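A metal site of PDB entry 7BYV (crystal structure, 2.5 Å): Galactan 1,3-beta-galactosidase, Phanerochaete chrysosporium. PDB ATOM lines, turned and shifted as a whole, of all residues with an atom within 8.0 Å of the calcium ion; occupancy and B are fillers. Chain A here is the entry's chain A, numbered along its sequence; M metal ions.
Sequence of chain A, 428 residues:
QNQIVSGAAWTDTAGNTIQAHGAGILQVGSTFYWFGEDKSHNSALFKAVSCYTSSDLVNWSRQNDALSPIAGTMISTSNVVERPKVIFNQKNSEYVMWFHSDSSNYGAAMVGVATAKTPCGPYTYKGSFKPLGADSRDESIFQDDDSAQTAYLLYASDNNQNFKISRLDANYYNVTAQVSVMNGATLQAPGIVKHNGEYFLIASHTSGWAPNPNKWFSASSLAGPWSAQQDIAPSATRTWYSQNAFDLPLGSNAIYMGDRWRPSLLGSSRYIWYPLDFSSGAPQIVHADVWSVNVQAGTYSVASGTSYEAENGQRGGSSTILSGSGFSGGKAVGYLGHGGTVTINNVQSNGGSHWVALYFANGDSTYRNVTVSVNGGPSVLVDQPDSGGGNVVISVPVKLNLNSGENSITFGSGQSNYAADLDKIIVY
Along chain A the residues within 4 Å of the calcium ion span positions 309 to 423.
The backbone carbonyl oxygen of Asp 423 lies close to the backbone NH of Ala 310 (3.1 Å). N of Asp 423 is in hydrogen-bond range of O of Tyr 359.
The calcium ion is bound by O of Ser 328, 2.3 Å away. The calcium ion is bound by OE1 of Glu 309, at 2.3 Å. The calcium ion is bound by OE1 of Glu 311 (2.3 Å). The calcium ion is bound by OD1 of Asp 423 (2.4 Å). The backbone carbonyl oxygen (O) of Lys 331 binds the calcium ion (2.4 Å). The backbone carbonyl oxygen (O) of Asp 423 binds the calcium ion, at 2.6 Å. The side-chain carboxylate (OE2) of Glu 311 binds the calcium ion, at 2.6 Å. The calcium ion has seven donor atoms within binding distance.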
ATOM      1  N   TYR A 308      -6.692 -15.404 -10.929  1.00  0.00           N
ATOM      2  CA  TYR A 308      -7.833 -15.729 -11.780  1.00  0.00           C
ATOM      3  C   TYR A 308      -7.436 -16.895 -12.672  1.00  0.00           C
ATOM      4  O   TYR A 308      -6.396 -16.840 -13.331  1.00  0.00           O
ATOM      5  CB  TYR A 308      -8.264 -14.523 -12.609  1.00  0.00           C
ATOM      6  CG  TYR A 308      -8.708 -13.346 -11.782  1.00  0.00           C
ATOM      7  CD1 TYR A 308      -7.794 -12.534 -11.140  1.00  0.00           C
ATOM      8  CD2 TYR A 308     -10.055 -13.033 -11.660  1.00  0.00           C
ATOM      9  CE1 TYR A 308      -8.219 -11.452 -10.385  1.00  0.00           C
ATOM     10  CE2 TYR A 308     -10.487 -11.962 -10.917  1.00  0.00           C
ATOM     11  CZ  TYR A 308      -9.574 -11.170 -10.282  1.00  0.00           C
ATOM     12  OH  TYR A 308     -10.028 -10.095  -9.537  1.00  0.00           O
ATOM     13  N   GLU A 309      -8.219 -17.963 -12.643  1.00  0.00           N
ATOM     14  CA  GLU A 309      -7.868 -19.138 -13.432  1.00  0.00           C
ATOM     15  C   GLU A 309      -8.237 -18.897 -14.884  1.00  0.00           C
ATOM     16  O   GLU A 309      -9.386 -18.545 -15.195  1.00  0.00           O
ATOM     17  CB  GLU A 309      -8.568 -20.383 -12.901  1.00  0.00           C
ATOM     18  CG  GLU A 309      -7.916 -21.015 -11.679  1.00  0.00           C
ATOM     19  CD  GLU A 309      -6.419 -21.414 -11.842  1.00  0.00           C
ATOM     20  OE1 GLU A 309      -5.832 -21.332 -12.961  1.00  0.00           O
ATOM     21  OE2 GLU A 309      -5.827 -21.814 -10.815  1.00  0.00           O
ATOM     22  N   ALA A 310      -7.267 -19.096 -15.783  1.00  0.00           N
ATOM     23  CA  ALA A 310      -7.545 -18.888 -17.201  1.00  0.00           C
ATOM     24  C   ALA A 310      -8.696 -19.767 -17.675  1.00  0.00           C
ATOM     25  O   ALA A 310      -9.527 -19.334 -18.478  1.00  0.00           O
ATOM     26  CB  ALA A 310      -6.280 -19.142 -18.011  1.00  0.00           C
ATOM     27  N   GLU A 311      -8.776 -20.989 -17.166  1.00  0.00           N
ATOM     28  CA  GLU A 311      -9.841 -21.914 -17.550  1.00  0.00           C
ATOM     29  C   GLU A 311     -11.234 -21.466 -17.089  1.00  0.00           C
ATOM     30  O   GLU A 311     -12.232 -21.943 -17.638  1.00  0.00           O
ATOM     31  CB  GLU A 311      -9.533 -23.307 -16.997  1.00  0.00           C
ATOM     32  CG  GLU A 311      -9.386 -23.372 -15.465  1.00  0.00           C
ATOM     33  CD  GLU A 311      -7.935 -23.288 -14.986  1.00  0.00           C
ATOM     34  OE1 GLU A 311      -7.126 -22.581 -15.625  1.00  0.00           O
ATOM     35  OE2 GLU A 311      -7.585 -23.922 -13.979  1.00  0.00           O
ATOM     36  N   ASN A 312     -11.337 -20.590 -16.101  1.00  0.00           N
ATOM     37  CA  ASN A 312     -12.624 -20.000 -15.736  1.00  0.00           C
ATOM     38  C   ASN A 312     -12.980 -18.825 -16.616  1.00  0.00           C
ATOM     39  O   ASN A 312     -14.099 -18.300 -16.498  1.00  0.00           O
ATOM     40  CB  ASN A 312     -12.653 -19.548 -14.275  1.00  0.00           C
ATOM     41  CG  ASN A 312     -12.542 -20.717 -13.311  1.00  0.00           C
ATOM     42  OD1 ASN A 312     -11.731 -20.677 -12.373  1.00  0.00           O
ATOM     43  ND2 ASN A 312     -13.329 -21.767 -13.541  1.00  0.00           N
ATOM     44  N   LEU A 322      -6.843 -27.434 -21.687  1.00  0.00           N
ATOM     45  CA  LEU A 322      -5.850 -28.484 -21.604  1.00  0.00           C
ATOM     46  C   LEU A 322      -5.643 -28.901 -20.162  1.00  0.00           C
ATOM     47  O   LEU A 322      -5.869 -28.121 -19.227  1.00  0.00           O
ATOM     48  CB  LEU A 322      -4.479 -28.075 -22.133  1.00  0.00           C
ATOM     49  CG  LEU A 322      -4.346 -27.167 -23.327  1.00  0.00           C
ATOM     50  CD1 LEU A 322      -2.907 -26.672 -23.414  1.00  0.00           C
ATOM     51  CD2 LEU A 322      -4.728 -27.974 -24.565  1.00  0.00           C
ATOM     52  N   GLY A 324      -3.027 -30.691 -17.236  1.00  0.00           N
ATOM     53  CA  GLY A 324      -1.666 -31.040 -16.904  1.00  0.00           C
ATOM     54  C   GLY A 324      -1.383 -30.812 -15.442  1.00  0.00           C
ATOM     55  O   GLY A 324      -1.912 -29.875 -14.844  1.00  0.00           O
ATOM     56  N   GLY A 326       1.176 -29.651 -14.208  1.00  0.00           N
ATOM     57  CA  GLY A 326       1.908 -28.415 -13.973  1.00  0.00           C
ATOM     58  C   GLY A 326       1.052 -27.171 -13.862  1.00  0.00           C
ATOM     59  O   GLY A 326       1.526 -26.142 -13.382  1.00  0.00           O
ATOM     60  N   PHE A 327      -0.203 -27.265 -14.290  1.00  0.00           N
ATOM     61  CA  PHE A 327      -1.097 -26.121 -14.295  1.00  0.00           C
ATOM     62  C   PHE A 327      -1.792 -25.969 -12.962  1.00  0.00           C
ATOM     63  O   PHE A 327      -2.168 -26.963 -12.315  1.00  0.00           O
ATOM     64  CB  PHE A 327      -2.163 -26.293 -15.368  1.00  0.00           C
ATOM     65  CG  PHE A 327      -1.626 -26.451 -16.744  1.00  0.00           C
ATOM     66  CD1 PHE A 327      -0.632 -25.602 -17.212  1.00  0.00           C
ATOM     67  CD2 PHE A 327      -2.129 -27.429 -17.588  1.00  0.00           C
ATOM     68  CE1 PHE A 327      -0.148 -25.748 -18.492  1.00  0.00           C
ATOM     69  CE2 PHE A 327      -1.648 -27.572 -18.858  1.00  0.00           C
ATOM     70  CZ  PHE A 327      -0.658 -26.722 -19.318  1.00  0.00           C
ATOM     71  N   SER A 328      -1.991 -24.728 -12.543  1.00  0.00           N
ATOM     72  CA  SER A 328      -2.795 -24.443 -11.371  1.00  0.00           C
ATOM     73  C   SER A 328      -4.259 -24.797 -11.655  1.00  0.00           C
ATOM     74  O   SER A 328      -4.817 -24.425 -12.695  1.00  0.00           O
ATOM     75  CB  SER A 328      -2.622 -22.978 -10.977  1.00  0.00           C
ATOM     76  OG  SER A 328      -3.686 -22.509 -10.184  1.00  0.00           O
ATOM     77  N   GLY A 329      -4.887 -25.512 -10.731  1.00  0.00           N
ATOM     78  CA  GLY A 329      -6.218 -26.031 -10.991  1.00  0.00           C
ATOM     79  C   GLY A 329      -6.246 -27.221 -11.901  1.00  0.00           C
ATOM     80  O   GLY A 329      -7.343 -27.713 -12.234  1.00  0.00           O
ATOM     81  N   GLY A 330      -5.084 -27.713 -12.328  1.00  0.00           N
ATOM     82  CA  GLY A 330      -5.002 -28.804 -13.258  1.00  0.00           C
ATOM     83  C   GLY A 330      -5.353 -28.451 -14.692  1.00  0.00           C
ATOM     84  O   GLY A 330      -5.333 -29.346 -15.546  1.00  0.00           O
ATOM     85  N   LYS A 331      -5.668 -27.200 -14.998  1.00  0.00           N
ATOM     86  CA  LYS A 331      -6.066 -26.870 -16.359  1.00  0.00           C
ATOM     87  C   LYS A 331      -5.378 -25.605 -16.833  1.00  0.00           C
ATOM     88  O   LYS A 331      -4.891 -24.792 -16.027  1.00  0.00           O
ATOM     89  CB  LYS A 331      -7.588 -26.741 -16.492  1.00  0.00           C
ATOM     90  CG  LYS A 331      -8.232 -28.013 -16.959  1.00  0.00           C
ATOM     91  CD  LYS A 331      -9.286 -28.510 -16.004  1.00  0.00           C
ATOM     92  CE  LYS A 331     -10.641 -27.860 -16.309  1.00  0.00           C
ATOM     93  NZ  LYS A 331     -11.663 -28.274 -15.302  1.00  0.00           N
ATOM     94  N   ALA A 332      -5.331 -25.457 -18.158  1.00  0.00           N
ATOM     95  CA  ALA A 332      -4.904 -24.226 -18.800  1.00  0.00           C
ATOM     96  C   ALA A 332      -5.676 -24.075 -20.114  1.00  0.00           C
ATOM     97  O   ALA A 332      -6.405 -24.976 -20.529  1.00  0.00           O
ATOM     98  CB  ALA A 332      -3.397 -24.215 -19.034  1.00  0.00           C
ATOM     99  N   VAL A 333      -5.531 -22.912 -20.739  1.00  0.00           N
ATOM    100  CA  VAL A 333      -6.183 -22.624 -22.010  1.00  0.00           C
ATOM    101  C   VAL A 333      -5.148 -22.720 -23.125  1.00  0.00           C
ATOM    102  O   VAL A 333      -4.186 -21.944 -23.172  1.00  0.00           O
ATOM    103  CB  VAL A 333      -6.863 -21.253 -22.007  1.00  0.00           C
ATOM    104  CG1 VAL A 333      -7.401 -20.931 -23.403  1.00  0.00           C
ATOM    105  CG2 VAL A 333      -7.991 -21.198 -20.945  1.00  0.00           C
ATOM    106  N   TYR A 359       0.702 -16.343 -16.020  1.00  0.00           N
ATOM    107  CA  TYR A 359       1.254 -17.671 -15.799  1.00  0.00           C
ATOM    108  C   TYR A 359       0.958 -18.533 -17.023  1.00  0.00           C
ATOM    109  O   TYR A 359      -0.201 -18.652 -17.427  1.00  0.00           O
ATOM    110  CB  TYR A 359       0.672 -18.299 -14.531  1.00  0.00           C
ATOM    111  CG  TYR A 359       1.339 -17.791 -13.277  1.00  0.00           C
ATOM    112  CD1 TYR A 359       1.166 -16.484 -12.872  1.00  0.00           C
ATOM    113  CD2 TYR A 359       2.166 -18.608 -12.506  1.00  0.00           C
ATOM    114  CE1 TYR A 359       1.777 -16.000 -11.724  1.00  0.00           C
ATOM    115  CE2 TYR A 359       2.768 -18.129 -11.339  1.00  0.00           C
ATOM    116  CZ  TYR A 359       2.567 -16.822 -10.968  1.00  0.00           C
ATOM    117  OH  TYR A 359       3.158 -16.317  -9.845  1.00  0.00           O
ATOM    118  N   VAL A 393       5.120 -24.225 -15.803  1.00  0.00           N
ATOM    119  CA  VAL A 393       4.551 -22.887 -15.813  1.00  0.00           C
ATOM    120  C   VAL A 393       5.551 -21.930 -15.198  1.00  0.00           C
ATOM    121  O   VAL A 393       6.018 -22.152 -14.085  1.00  0.00           O
ATOM    122  CB  VAL A 393       3.207 -22.856 -15.090  1.00  0.00           C
ATOM    123  CG1 VAL A 393       2.790 -21.395 -14.808  1.00  0.00           C
ATOM    124  CG2 VAL A 393       2.169 -23.609 -15.929  1.00  0.00           C
ATOM    125  N   LEU A 422      -2.191 -20.396 -21.448  1.00  0.00           N
ATOM    126  CA  LEU A 422      -2.385 -19.560 -20.269  1.00  0.00           C
ATOM    127  C   LEU A 422      -2.916 -20.395 -19.102  1.00  0.00           C
ATOM    128  O   LEU A 422      -4.017 -20.965 -19.178  1.00  0.00           O
ATOM    129  CB  LEU A 422      -3.336 -18.412 -20.565  1.00  0.00           C
ATOM    130  CG  LEU A 422      -3.301 -17.251 -19.557  1.00  0.00           C
ATOM    131  CD1 LEU A 422      -1.892 -16.715 -19.367  1.00  0.00           C
ATOM    132  CD2 LEU A 422      -4.218 -16.148 -19.994  1.00  0.00           C
ATOM    133  N   ASP A 423      -2.137 -20.455 -18.024  1.00  0.00           N
ATOM    134  CA  ASP A 423      -2.532 -21.166 -16.804  1.00  0.00           C
ATOM    135  C   ASP A 423      -3.491 -20.319 -15.958  1.00  0.00           C
ATOM    136  O   ASP A 423      -4.612 -20.754 -15.651  1.00  0.00           O
ATOM    137  CB  ASP A 423      -1.288 -21.544 -15.996  1.00  0.00           C
ATOM    138  CG  ASP A 423      -1.612 -22.402 -14.781  1.00  0.00           C
ATOM    139  OD1 ASP A 423      -2.781 -22.852 -14.668  1.00  0.00           O
ATOM    140  OD2 ASP A 423      -0.723 -22.624 -13.922  1.00  0.00           O
ATOM    141  N   LYS A 424      -3.070 -19.112 -15.605  1.00  0.00           N
ATOM    142  CA  LYS A 424      -3.800 -18.221 -14.716  1.00  0.00           C
ATOM    143  C   LYS A 424      -3.149 -16.859 -14.807  1.00  0.00           C
ATOM    144  O   LYS A 424      -2.102 -16.700 -15.451  1.00  0.00           O
ATOM    145  CB  LYS A 424      -3.784 -18.724 -13.269  1.00  0.00           C
ATOM    146  CG  LYS A 424      -2.419 -18.540 -12.615  1.00  0.00           C
ATOM    147  CD  LYS A 424      -2.226 -19.538 -11.487  1.00  0.00           C
ATOM    148  CE  LYS A 424      -1.402 -18.969 -10.323  1.00  0.00           C
ATOM    149  NZ  LYS A 424      -2.252 -18.572  -9.139  1.00  0.00           N
ATOM    150  N   ILE A 425      -3.763 -15.877 -14.153  1.00  0.00           N
ATOM    151  CA  ILE A 425      -3.122 -14.587 -13.946  1.00  0.00           C
ATOM    152  C   ILE A 425      -3.253 -14.239 -12.484  1.00  0.00           C
ATOM    153  O   ILE A 425      -4.159 -14.714 -11.781  1.00  0.00           O
ATOM    154  CB  ILE A 425      -3.701 -13.474 -14.840  1.00  0.00           C
ATOM    155  CG1 ILE A 425      -5.200 -13.333 -14.602  1.00  0.00           C
ATOM    156  CG2 ILE A 425      -3.460 -13.780 -16.287  1.00  0.00           C
ATOM    157  CD1 ILE A 425      -5.696 -12.021 -15.029  1.00  0.00           C
HETATM  158 CA    CA M   1      -5.160 -22.986 -14.442  1.00  0.00          CA
